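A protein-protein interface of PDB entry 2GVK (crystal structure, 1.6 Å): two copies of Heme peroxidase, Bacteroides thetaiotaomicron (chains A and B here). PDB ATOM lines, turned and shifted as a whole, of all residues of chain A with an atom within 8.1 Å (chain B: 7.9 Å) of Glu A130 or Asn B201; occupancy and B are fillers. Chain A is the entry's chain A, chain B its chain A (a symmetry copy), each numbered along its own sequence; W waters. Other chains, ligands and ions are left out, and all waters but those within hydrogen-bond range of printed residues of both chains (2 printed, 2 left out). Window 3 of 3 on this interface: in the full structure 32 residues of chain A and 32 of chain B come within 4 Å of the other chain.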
ATOM      1  N   TYR A  30      10.559 -10.954   9.253  1.00  0.00           N
ATOM      2  CA  TYR A  30      11.037 -10.304  10.456  1.00  0.00           C
ATOM      3  C   TYR A  30      12.300 -10.984  10.957  1.00  0.00           C
ATOM      4  O   TYR A  30      12.437 -12.206  10.851  1.00  0.00           O
ATOM      5  CB  TYR A  30      10.007 -10.442  11.565  1.00  0.00           C
ATOM      6  CG  TYR A  30       8.774  -9.571  11.468  1.00  0.00           C
ATOM      7  CD1 TYR A  30       8.875  -8.205  11.511  1.00  0.00           C
ATOM      8  CD2 TYR A  30       7.502 -10.130  11.608  1.00  0.00           C
ATOM      9  CE1 TYR A  30       7.734  -7.391  11.583  1.00  0.00           C
ATOM     10  CE2 TYR A  30       6.369  -9.329  11.671  1.00  0.00           C
ATOM     11  CZ  TYR A  30       6.498  -7.963  11.653  1.00  0.00           C
ATOM     12  OH  TYR A  30       5.389  -7.160  11.780  1.00  0.00           O
ATOM     13  N   LYS A  41       6.318 -13.082  23.182  1.00  0.00           N
ATOM     14  CA  LYS A  41       5.479 -12.406  22.179  1.00  0.00           C
ATOM     15  C   LYS A  41       5.308 -13.273  20.937  1.00  0.00           C
ATOM     16  O   LYS A  41       4.206 -13.384  20.396  1.00  0.00           O
ATOM     17  CB  LYS A  41       6.040 -11.024  21.838  1.00  0.00           C
ATOM     18  CG  LYS A  41       5.816 -10.035  22.969  1.00  0.00           C
ATOM     19  CD  LYS A  41       6.374  -8.692  22.685  1.00  0.00           C
ATOM     20  CE  LYS A  41       6.125  -7.747  23.856  1.00  0.00           C
ATOM     21  NZ  LYS A  41       6.963  -6.528  23.757  1.00  0.00           N
ATOM     22  N   ASP A  44       2.857 -15.969  21.846  1.00  0.00           N
ATOM     23  CA  ASP A  44       1.468 -15.406  21.861  1.00  0.00           C
ATOM     24  C   ASP A  44       0.869 -15.455  20.483  1.00  0.00           C
ATOM     25  O   ASP A  44      -0.283 -15.816  20.306  1.00  0.00           O
ATOM     26  CB  ASP A  44       1.447 -13.953  22.354  1.00  0.00           C
ATOM     27  CG  ASP A  44       0.019 -13.334  22.312  1.00  0.00           C
ATOM     28  OD1 ASP A  44      -0.841 -13.772  23.126  1.00  0.00           O
ATOM     29  OD2 ASP A  44      -0.239 -12.424  21.471  1.00  0.00           O
ATOM     30  N   VAL A  45       1.656 -15.090  19.484  1.00  0.00           N
ATOM     31  CA  VAL A  45       1.173 -15.162  18.101  1.00  0.00           C
ATOM     32  C   VAL A  45       0.925 -16.636  17.697  1.00  0.00           C
ATOM     33  O   VAL A  45      -0.111 -16.960  17.130  1.00  0.00           O
ATOM     34  CB  VAL A  45       2.148 -14.489  17.106  1.00  0.00           C
ATOM     35  CG1 VAL A  45       1.718 -14.755  15.676  1.00  0.00           C
ATOM     36  CG2 VAL A  45       2.215 -13.007  17.354  1.00  0.00           C
ATOM     37  N   PHE A 122      -4.013  -6.115   5.397  1.00  0.00           N
ATOM     38  CA  PHE A 122      -3.543  -5.053   6.287  1.00  0.00           C
ATOM     39  C   PHE A 122      -4.045  -5.265   7.698  1.00  0.00           C
ATOM     40  O   PHE A 122      -3.301  -5.139   8.641  1.00  0.00           O
ATOM     41  CB  PHE A 122      -3.987  -3.655   5.791  1.00  0.00           C
ATOM     42  CG  PHE A 122      -3.925  -2.607   6.847  1.00  0.00           C
ATOM     43  CD1 PHE A 122      -2.718  -2.049   7.211  1.00  0.00           C
ATOM     44  CD2 PHE A 122      -5.070  -2.236   7.558  1.00  0.00           C
ATOM     45  CE1 PHE A 122      -2.650  -1.134   8.231  1.00  0.00           C
ATOM     46  CE2 PHE A 122      -5.007  -1.289   8.567  1.00  0.00           C
ATOM     47  CZ  PHE A 122      -3.789  -0.762   8.921  1.00  0.00           C
ATOM     48  N   GLU A 123      -5.311  -5.595   7.839  1.00  0.00           N
ATOM     49  CA  GLU A 123      -5.902  -5.773   9.159  1.00  0.00           C
ATOM     50  C   GLU A 123      -5.111  -6.822   9.966  1.00  0.00           C
ATOM     51  O   GLU A 123      -4.685  -6.574  11.107  1.00  0.00           O
ATOM     52  CB  GLU A 123      -7.378  -6.197   9.014  1.00  0.00           C
ATOM     53  CG  GLU A 123      -8.064  -6.595  10.313  1.00  0.00           C
ATOM     54  CD  GLU A 123      -8.520  -5.426  11.100  1.00  0.00           C
ATOM     55  OE1 GLU A 123      -7.970  -4.314  10.894  1.00  0.00           O
ATOM     56  OE2 GLU A 123      -9.488  -5.588  11.887  1.00  0.00           O
ATOM     57  N   PHE A 124      -4.914  -7.974   9.367  1.00  0.00           N
ATOM     58  CA  PHE A 124      -4.195  -9.064  10.001  1.00  0.00           C
ATOM     59  C   PHE A 124      -2.757  -8.640  10.330  1.00  0.00           C
ATOM     60  O   PHE A 124      -2.278  -8.838  11.437  1.00  0.00           O
ATOM     61  CB  PHE A 124      -4.191 -10.278   9.062  1.00  0.00           C
ATOM     62  CG  PHE A 124      -3.833 -11.593   9.747  1.00  0.00           C
ATOM     63  CD1 PHE A 124      -2.518 -11.957   9.910  1.00  0.00           C
ATOM     64  CD2 PHE A 124      -4.840 -12.468  10.207  1.00  0.00           C
ATOM     65  CE1 PHE A 124      -2.187 -13.172  10.490  1.00  0.00           C
ATOM     66  CE2 PHE A 124      -4.519 -13.660  10.772  1.00  0.00           C
ATOM     67  CZ  PHE A 124      -3.190 -14.030  10.907  1.00  0.00           C
ATOM     68  N   ALA A 125      -2.090  -8.025   9.363  1.00  0.00           N
ATOM     69  CA  ALA A 125      -0.732  -7.602   9.554  1.00  0.00           C
ATOM     70  C   ALA A 125      -0.589  -6.560  10.677  1.00  0.00           C
ATOM     71  O   ALA A 125       0.395  -6.568  11.395  1.00  0.00           O
ATOM     72  CB  ALA A 125      -0.152  -7.065   8.236  1.00  0.00           C
ATOM     73  N   SER A 126      -1.577  -5.678  10.824  1.00  0.00           N
ATOM     74  CA  SER A 126      -1.525  -4.659  11.857  1.00  0.00           C
ATOM     75  C   SER A 126      -1.615  -5.301  13.248  1.00  0.00           C
ATOM     76  O   SER A 126      -0.967  -4.851  14.187  1.00  0.00           O
ATOM     77  CB  SER A 126      -2.637  -3.604  11.657  1.00  0.00           C
ATOM     78  OG  SER A 126      -3.910  -4.105  12.017  1.00  0.00           O
ATOM     79  N   ILE A 127      -2.397  -6.363  13.361  1.00  0.00           N
ATOM     80  CA  ILE A 127      -2.526  -7.051  14.631  1.00  0.00           C
ATOM     81  C   ILE A 127      -1.205  -7.777  14.965  1.00  0.00           C
ATOM     82  O   ILE A 127      -0.755  -7.740  16.099  1.00  0.00           O
ATOM     83  CB  ILE A 127      -3.731  -7.993  14.631  1.00  0.00           C
ATOM     84  CG1 ILE A 127      -5.035  -7.155  14.548  1.00  0.00           C
ATOM     85  CG2 ILE A 127      -3.734  -8.851  15.878  1.00  0.00           C
ATOM     86  CD1 ILE A 127      -6.237  -7.927  14.119  1.00  0.00           C
ATOM     87  N   LEU A 128      -0.552  -8.350  13.944  1.00  0.00           N
ATOM     88  CA  LEU A 128       0.789  -8.959  14.129  1.00  0.00           C
ATOM     89  C   LEU A 128       1.787  -7.903  14.620  1.00  0.00           C
ATOM     90  O   LEU A 128       2.572  -8.152  15.530  1.00  0.00           O
ATOM     91  CB  LEU A 128       1.301  -9.580  12.821  1.00  0.00           C
ATOM     92  CG  LEU A 128       0.555 -10.791  12.299  1.00  0.00           C
ATOM     93  CD1 LEU A 128       1.101 -11.182  10.922  1.00  0.00           C
ATOM     94  CD2 LEU A 128       0.652 -11.958  13.265  1.00  0.00           C
ATOM     95  N   ASP A 129       1.727  -6.711  14.018  1.00  0.00           N
ATOM     96  CA  ASP A 129       2.604  -5.597  14.414  1.00  0.00           C
ATOM     97  C   ASP A 129       2.427  -5.292  15.902  1.00  0.00           C
ATOM     98  O   ASP A 129       3.403  -5.167  16.647  1.00  0.00           O
ATOM     99  CB  ASP A 129       2.278  -4.360  13.556  1.00  0.00           C
ATOM    100  CG  ASP A 129       3.104  -3.117  13.949  1.00  0.00           C
ATOM    101  OD1 ASP A 129       4.328  -3.247  14.246  1.00  0.00           O
ATOM    102  OD2 ASP A 129       2.530  -1.985  13.887  1.00  0.00           O
ATOM    103  N   GLU A 130       1.176  -5.180  16.323  1.00  0.00           N
ATOM    104  CA  GLU A 130       0.844  -4.898  17.714  1.00  0.00           C
ATOM    105  C   GLU A 130       1.309  -6.003  18.658  1.00  0.00           C
ATOM    106  O   GLU A 130       1.903  -5.732  19.701  1.00  0.00           O
ATOM    107  CB  GLU A 130      -0.667  -4.700  17.868  1.00  0.00           C
ATOM    108  CG  GLU A 130      -1.182  -3.416  17.216  1.00  0.00           C
ATOM    109  CD  GLU A 130      -2.713  -3.411  16.997  1.00  0.00           C
ATOM    110  OE1 GLU A 130      -3.395  -4.414  17.366  1.00  0.00           O
ATOM    111  OE2 GLU A 130      -3.211  -2.426  16.414  1.00  0.00           O
ATOM    112  N   LYS A 131       1.047  -7.245  18.288  1.00  0.00           N
ATOM    113  CA  LYS A 131       1.385  -8.373  19.147  1.00  0.00           C
ATOM    114  C   LYS A 131       2.889  -8.595  19.251  1.00  0.00           C
ATOM    115  O   LYS A 131       3.385  -9.092  20.284  1.00  0.00           O
ATOM    116  CB  LYS A 131       0.703  -9.647  18.643  1.00  0.00           C
ATOM    117  CG  LYS A 131      -0.781  -9.733  18.930  1.00  0.00           C
ATOM    118  CD  LYS A 131      -1.340 -11.118  18.419  1.00  0.00           C
ATOM    119  CE  LYS A 131      -2.800 -11.309  18.764  1.00  0.00           C
ATOM    120  NZ  LYS A 131      -3.004 -11.335  20.229  1.00  0.00           N
ATOM    121  N   LEU A 132       3.626  -8.236  18.208  1.00  0.00           N
ATOM    122  CA  LEU A 132       5.063  -8.506  18.169  1.00  0.00           C
ATOM    123  C   LEU A 132       5.911  -7.289  18.496  1.00  0.00           C
ATOM    124  O   LEU A 132       7.138  -7.355  18.422  1.00  0.00           O
ATOM    125  CB  LEU A 132       5.459  -9.044  16.790  1.00  0.00           C
ATOM    126  CG  LEU A 132       4.898 -10.431  16.463  1.00  0.00           C
ATOM    127  CD1 LEU A 132       5.060 -10.756  14.981  1.00  0.00           C
ATOM    128  CD2 LEU A 132       5.564 -11.496  17.330  1.00  0.00           C
ATOM    129  N   LYS A 133       5.265  -6.198  18.927  1.00  0.00           N
ATOM    130  CA  LYS A 133       5.970  -4.937  19.190  1.00  0.00           C
ATOM    131  C   LYS A 133       7.136  -5.150  20.156  1.00  0.00           C
ATOM    132  O   LYS A 133       6.944  -5.621  21.266  1.00  0.00           O
ATOM    133  CB  LYS A 133       4.991  -3.891  19.765  1.00  0.00           C
ATOM    134  CG  LYS A 133       5.519  -2.484  19.751  1.00  0.00           C
ATOM    135  CD  LYS A 133       5.427  -1.873  18.355  1.00  0.00           C
ATOM    136  N   GLY A 134       8.343  -4.797  19.709  1.00  0.00           N
ATOM    137  CA  GLY A 134       9.549  -4.907  20.537  1.00  0.00           C
ATOM    138  C   GLY A 134      10.294  -6.211  20.353  1.00  0.00           C
ATOM    139  O   GLY A 134      11.480  -6.308  20.698  1.00  0.00           O
ATOM    140  N   ALA A 135       9.609  -7.201  19.793  1.00  0.00           N
ATOM    141  CA  ALA A 135      10.155  -8.571  19.614  1.00  0.00           C
ATOM    142  C   ALA A 135      10.771  -8.775  18.240  1.00  0.00           C
ATOM    143  O   ALA A 135      11.540  -9.749  18.022  1.00  0.00           O
ATOM    144  CB  ALA A 135       9.049  -9.594  19.834  1.00  0.00           C
ATOM    145  N   VAL A 136      10.450  -7.885  17.311  1.00  0.00           N
ATOM    146  CA  VAL A 136      10.896  -8.039  15.930  1.00  0.00           C
ATOM    147  C   VAL A 136      11.333  -6.740  15.274  1.00  0.00           C
ATOM    148  O   VAL A 136      10.976  -5.637  15.726  1.00  0.00           O
ATOM    149  CB  VAL A 136       9.744  -8.659  15.011  1.00  0.00           C
ATOM    150  CG1 VAL A 136       9.387 -10.071  15.469  1.00  0.00           C
ATOM    151  CG2 VAL A 136       8.535  -7.766  14.998  1.00  0.00           C
ATOM    152  N   ILE B 153      -7.553   4.834   8.067  1.00  0.00           N
ATOM    153  CA  ILE B 153      -6.692   3.889   8.746  1.00  0.00           C
ATOM    154  C   ILE B 153      -6.797   4.034  10.295  1.00  0.00           C
ATOM    155  O   ILE B 153      -6.453   3.110  11.040  1.00  0.00           O
ATOM    156  CB  ILE B 153      -5.238   4.049   8.246  1.00  0.00           C
ATOM    157  CG1 ILE B 153      -4.427   2.756   8.470  1.00  0.00           C
ATOM    158  CG2 ILE B 153      -4.579   5.253   8.884  1.00  0.00           C
ATOM    159  CD1 ILE B 153      -3.145   2.726   7.684  1.00  0.00           C
ATOM    160  N   ILE B 154      -7.324   5.173  10.748  1.00  0.00           N
ATOM    161  CA  ILE B 154      -7.599   5.406  12.189  1.00  0.00           C
ATOM    162  C   ILE B 154      -8.928   4.743  12.660  1.00  0.00           C
ATOM    163  O   ILE B 154      -9.333   4.907  13.804  1.00  0.00           O
ATOM    164  CB  ILE B 154      -7.643   6.914  12.512  1.00  0.00           C
ATOM    165  CG1 ILE B 154      -8.615   7.621  11.544  1.00  0.00           C
ATOM    166  CG2 ILE B 154      -6.275   7.487  12.418  1.00  0.00           C
ATOM    167  CD1 ILE B 154      -9.183   8.851  12.063  1.00  0.00           C
ATOM    168  N   GLY B 155      -9.609   4.045  11.754  1.00  0.00           N
ATOM    169  CA  GLY B 155     -10.743   3.185  12.122  1.00  0.00           C
ATOM    170  C   GLY B 155     -12.083   3.845  12.120  1.00  0.00           C
ATOM    171  O   GLY B 155     -13.035   3.314  12.673  1.00  0.00           O
ATOM    172  N   ASP B 196       0.581   8.668  14.451  1.00  0.00           N
ATOM    173  CA  ASP B 196       1.084   8.103  15.695  1.00  0.00           C
ATOM    174  C   ASP B 196       0.018   7.138  16.178  1.00  0.00           C
ATOM    175  O   ASP B 196      -0.861   7.491  16.961  1.00  0.00           O
ATOM    176  CB  ASP B 196       1.323   9.215  16.713  1.00  0.00           C
ATOM    177  CG  ASP B 196       1.973   8.718  18.000  1.00  0.00           C
ATOM    178  OD1 ASP B 196       2.005   7.477  18.241  1.00  0.00           O
ATOM    179  OD2 ASP B 196       2.420   9.588  18.804  1.00  0.00           O
ATOM    180  N   MET B 197       0.068   5.918  15.650  1.00  0.00           N
ATOM    181  CA  MET B 197      -0.972   4.907  15.940  1.00  0.00           C
ATOM    182  C   MET B 197      -0.941   4.417  17.362  1.00  0.00           C
ATOM    183  O   MET B 197      -1.961   4.072  17.913  1.00  0.00           O
ATOM    184  CB  MET B 197      -0.849   3.722  14.989  1.00  0.00           C
ATOM    185  CG  MET B 197      -1.127   4.068  13.601  1.00  0.00           C
ATOM    186  SD  MET B 197      -2.920   4.829  13.351  1.00  0.00           S
ATOM    187  CE  MET B 197      -3.930   3.177  13.234  1.00  0.00           C
ATOM    188  N   VAL B 198       0.222   4.416  17.980  1.00  0.00           N
ATOM    189  CA  VAL B 198       0.312   3.985  19.357  1.00  0.00           C
ATOM    190  C   VAL B 198      -0.448   4.957  20.269  1.00  0.00           C
ATOM    191  O   VAL B 198      -1.291   4.545  21.058  1.00  0.00           O
ATOM    192  CB  VAL B 198       1.785   3.838  19.808  1.00  0.00           C
ATOM    193  CG1 VAL B 198       1.861   3.614  21.283  1.00  0.00           C
ATOM    194  CG2 VAL B 198       2.442   2.689  19.047  1.00  0.00           C
ATOM    195  N   ALA B 199      -0.241   6.249  20.066  1.00  0.00           N
ATOM    196  CA  ALA B 199      -0.952   7.253  20.846  1.00  0.00           C
ATOM    197  C   ALA B 199      -2.461   7.221  20.548  1.00  0.00           C
ATOM    198  O   ALA B 199      -3.275   7.373  21.450  1.00  0.00           O
ATOM    199  CB  ALA B 199      -0.405   8.592  20.566  1.00  0.00           C
ATOM    200  N   TRP B 200      -2.817   7.060  19.269  1.00  0.00           N
ATOM    201  CA  TRP B 200      -4.222   7.018  18.857  1.00  0.00           C
ATOM    202  C   TRP B 200      -4.952   5.850  19.491  1.00  0.00           C
ATOM    203  O   TRP B 200      -6.051   6.004  20.017  1.00  0.00           O
ATOM    204  CB  TRP B 200      -4.315   6.922  17.340  1.00  0.00           C
ATOM    205  CG  TRP B 200      -5.698   6.810  16.821  1.00  0.00           C
ATOM    206  CD1 TRP B 200      -6.258   5.726  16.232  1.00  0.00           C
ATOM    207  CD2 TRP B 200      -6.715   7.835  16.835  1.00  0.00           C
ATOM    208  NE1 TRP B 200      -7.555   5.987  15.901  1.00  0.00           N
ATOM    209  CE2 TRP B 200      -7.855   7.288  16.232  1.00  0.00           C
ATOM    210  CE3 TRP B 200      -6.765   9.157  17.311  1.00  0.00           C
ATOM    211  CZ2 TRP B 200      -9.039   8.024  16.058  1.00  0.00           C
ATOM    212  CZ3 TRP B 200      -7.944   9.885  17.139  1.00  0.00           C
ATOM    213  CH2 TRP B 200      -9.065   9.308  16.540  1.00  0.00           C
ATOM    214  N   ASN B 201      -4.325   4.681  19.452  1.00  0.00           N
ATOM    215  CA  ASN B 201      -4.947   3.469  19.952  1.00  0.00           C
ATOM    216  C   ASN B 201      -5.060   3.481  21.491  1.00  0.00           C
ATOM    217  O   ASN B 201      -5.846   2.755  22.059  1.00  0.00           O
ATOM    218  CB  ASN B 201      -4.165   2.228  19.476  1.00  0.00           C
ATOM    219  CG  ASN B 201      -4.397   1.902  17.988  1.00  0.00           C
ATOM    220  OD1 ASN B 201      -5.424   2.247  17.413  1.00  0.00           O
ATOM    221  ND2 ASN B 201      -3.491   1.142  17.413  1.00  0.00           N
ATOM    222  N   ALA B 202      -4.289   4.338  22.141  1.00  0.00           N
ATOM    223  CA  ALA B 202      -4.349   4.468  23.585  1.00  0.00           C
ATOM    224  C   ALA B 202      -5.561   5.297  24.039  1.00  0.00           C
ATOM    225  O   ALA B 202      -5.902   5.310  25.235  1.00  0.00           O
ATOM    226  CB  ALA B 202      -3.048   5.090  24.116  1.00  0.00           C
ATOM    227  N   LEU B 203      -6.179   6.032  23.103  1.00  0.00           N
ATOM    228  CA  LEU B 203      -7.381   6.831  23.400  1.00  0.00           C
ATOM    229  C   LEU B 203      -8.608   5.959  23.490  1.00  0.00           C
ATOM    230  O   LEU B 203      -8.839   5.126  22.616  1.00  0.00           O
ATOM    231  CB  LEU B 203      -7.630   7.855  22.296  1.00  0.00           C
ATOM    232  CG  LEU B 203      -6.810   9.110  22.260  1.00  0.00           C
ATOM    233  CD1 LEU B 203      -7.248   9.942  21.056  1.00  0.00           C
ATOM    234  CD2 LEU B 203      -6.970   9.906  23.572  1.00  0.00           C
ATOM    235  N   PRO B 204      -9.437   6.164  24.531  1.00  0.00           N
ATOM    236  CA  PRO B 204     -10.699   5.467  24.530  1.00  0.00           C
ATOM    237  C   PRO B 204     -11.545   5.916  23.345  1.00  0.00           C
ATOM    238  O   PRO B 204     -11.359   7.025  22.826  1.00  0.00           O
ATOM    239  CB  PRO B 204     -11.356   5.909  25.842  1.00  0.00           C
ATOM    240  CG  PRO B 204     -10.296   6.500  26.630  1.00  0.00           C
ATOM    241  CD  PRO B 204      -9.285   7.023  25.702  1.00  0.00           C
ATOM    242  N   VAL B 205     -12.471   5.089  22.935  1.00  0.00           N
ATOM    243  CA  VAL B 205     -13.274   5.383  21.765  1.00  0.00           C
ATOM    244  C   VAL B 205     -14.018   6.718  21.907  1.00  0.00           C
ATOM    245  O   VAL B 205     -14.110   7.484  20.967  1.00  0.00           O
ATOM    246  CB  VAL B 205     -14.283   4.272  21.490  1.00  0.00           C
ATOM    247  CG1 VAL B 205     -15.311   4.707  20.403  1.00  0.00           C
ATOM    248  CG2 VAL B 205     -13.554   2.975  21.070  1.00  0.00           C
ATOM    249  N   GLN B 208     -11.711   9.385  20.998  1.00  0.00           N
ATOM    250  CA  GLN B 208     -11.455   9.332  19.556  1.00  0.00           C
ATOM    251  C   GLN B 208     -12.612   9.993  18.805  1.00  0.00           C
ATOM    252  O   GLN B 208     -12.402  10.703  17.833  1.00  0.00           O
ATOM    253  CB  GLN B 208     -11.291   7.892  19.060  1.00  0.00           C
ATOM    254  CG  GLN B 208      -9.995   7.220  19.466  1.00  0.00           C
ATOM    255  CD  GLN B 208      -9.872   5.824  18.884  1.00  0.00           C
ATOM    256  OE1 GLN B 208     -10.828   5.290  18.331  1.00  0.00           O
ATOM    257  NE2 GLN B 208      -8.691   5.215  19.028  1.00  0.00           N
ATOM    258  N   LYS B 216     -17.912   6.205  16.120  1.00  0.00           N
ATOM    259  CA  LYS B 216     -17.001   5.305  15.479  1.00  0.00           C
ATOM    260  C   LYS B 216     -17.709   4.155  14.772  1.00  0.00           C
ATOM    261  O   LYS B 216     -17.328   3.770  13.653  1.00  0.00           O
ATOM    262  CB  LYS B 216     -15.987   4.745  16.490  1.00  0.00           C
ATOM    263  CG  LYS B 216     -14.817   3.984  15.817  1.00  0.00           C
ATOM    264  CD  LYS B 216     -13.723   3.675  16.794  1.00  0.00           C
ATOM    265  CE  LYS B 216     -12.483   3.074  16.109  1.00  0.00           C
ATOM    266  NZ  LYS B 216     -11.324   2.863  17.086  1.00  0.00           N
ATOM    267  N   THR B 254       3.169  -2.149   7.859  1.00  0.00           N
ATOM    268  CA  THR B 254       2.982  -2.506   9.265  1.00  0.00           C
ATOM    269  C   THR B 254       4.219  -3.140   9.899  1.00  0.00           C
ATOM    270  O   THR B 254       4.430  -3.018  11.075  1.00  0.00           O
ATOM    271  CB  THR B 254       1.789  -3.437   9.455  1.00  0.00           C
ATOM    272  OG1 THR B 254       1.978  -4.621   8.689  1.00  0.00           O
ATOM    273  CG2 THR B 254       0.510  -2.752   9.010  1.00  0.00           C
ATOM    274  N   GLY B 257       5.933  -0.558  11.436  1.00  0.00           N
ATOM    275  CA  GLY B 257       5.056   0.245  12.269  1.00  0.00           C
ATOM    276  C   GLY B 257       4.634   1.549  11.609  1.00  0.00           C
ATOM    277  O   GLY B 257       4.327   2.517  12.295  1.00  0.00           O
ATOM    278  N   TYR B 259       2.053   3.740   9.536  1.00  0.00           N
ATOM    279  CA  TYR B 259       0.638   3.857   9.204  1.00  0.00           C
ATOM    280  C   TYR B 259       0.376   5.264   8.732  1.00  0.00           C
ATOM    281  O   TYR B 259       0.762   6.236   9.412  1.00  0.00           O
ATOM    282  CB  TYR B 259      -0.235   3.578  10.408  1.00  0.00           C
ATOM    283  CG  TYR B 259      -0.088   2.184  10.972  1.00  0.00           C
ATOM    284  CD1 TYR B 259       0.953   1.870  11.826  1.00  0.00           C
ATOM    285  CD2 TYR B 259      -1.016   1.208  10.694  1.00  0.00           C
ATOM    286  CE1 TYR B 259       1.105   0.598  12.325  1.00  0.00           C
ATOM    287  CE2 TYR B 259      -0.892  -0.064  11.227  1.00  0.00           C
ATOM    288  CZ  TYR B 259       0.171  -0.356  12.041  1.00  0.00           C
ATOM    289  OH  TYR B 259       0.309  -1.646  12.543  1.00  0.00           O
ATOM    290  N   PHE B 295      -2.245  13.603  16.173  1.00  0.00           N
ATOM    291  CA  PHE B 295      -1.963  12.198  15.899  1.00  0.00           C
ATOM    292  C   PHE B 295      -1.516  11.969  14.477  1.00  0.00           C
ATOM    293  O   PHE B 295      -1.323  10.817  14.059  1.00  0.00           O
ATOM    294  CB  PHE B 295      -3.208  11.349  16.184  1.00  0.00           C
ATOM    295  CG  PHE B 295      -3.712  11.486  17.553  1.00  0.00           C
ATOM    296  CD1 PHE B 295      -3.213  10.691  18.575  1.00  0.00           C
ATOM    297  CD2 PHE B 295      -4.671  12.448  17.864  1.00  0.00           C
ATOM    298  CE1 PHE B 295      -3.670  10.844  19.863  1.00  0.00           C
ATOM    299  CE2 PHE B 295      -5.116  12.608  19.153  1.00  0.00           C
ATOM    300  CZ  PHE B 295      -4.624  11.799  20.151  1.00  0.00           C
HETATM  301  O   HOH W   1       3.005  -6.503  10.460  1.00  0.00           O
HETATM  302  O   HOH W   2       5.939  -4.998  13.174  1.00  0.00           O
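Among the printed residues, pairs that only touch across the chains: Ala A125 with Thr B254 (3.3 Å), Ser A126 with Tyr B259 (3.6 Å), Phe A122 with Ile B153 (3.6 Å), Phe A122 with Thr B254 (3.6 Å), Phe A122 with Tyr B259 (3.6 Å), Glu A130 with Asn B201 (3.7 Å), Asp A129 with Gly B257 (3.7 Å) and Ser A126 with Thr B254 (3.99 Å).
Printed residues of chain A that touch a printed residue of chain B: Phe A122, Ala A125, Ser A126, Asp A129 and Glu A130. Hydrophobic or aromatic side chains of chain A within 4 Å of the printed part of chain B: Phe A122 and Ala A125. Among the printed residues, no Asp or Glu carboxylate lies within 4 Å of a Lys or Arg side-chain nitrogen of the other chain.
OD2 of Asp A129 lies within hydrogen-bond range of OH of Tyr B259 (2.6 Å). OD1 of Asp A129 lies close to O of Thr B254, 3.2 Å away.
The side-chain hydroxyl of Ser A126 is in hydrogen-bond range of the backbone carbonyl oxygen of Glu A123 (2.7 Å). The backbone carbonyl oxygen (O) of Met B197 sits close to the side-chain amide nitrogen (ND2) of Asn B201 (3.3 Å).
Water W2 lies within hydrogen-bond range of OD1 of Asp A129 (2.6 Å), OH of Tyr A30 (2.6 Å) and O of Thr B254 (3.3 Å). Water W1 lies within hydrogen-bond range of O of Ala A125 (2.8 Å), OG1 of Thr B254 (2.8 Å) and OH of Tyr A30 (2.8 Å).
Glu A130 touches one residue of chain B. Asn B201 touches one residue of chain A. Of the printed residues of chain A, Ile B153 touches Phe A122 (3.6 Å). Printed residues of chain A within 4 Å of Gly B257: Asp A129 (3.7 Å). Of the printed residues of chain B, Ser A126 touches Thr B254 and Tyr B259. The nearest printed residue of chain B that does not touch Ser A126 is Met B197 (7.1 Å).
No position is printed for both chains. Of the 10 pairs that touch across the chains among the printed residues, none has its exchanged pair printed and touching as well.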
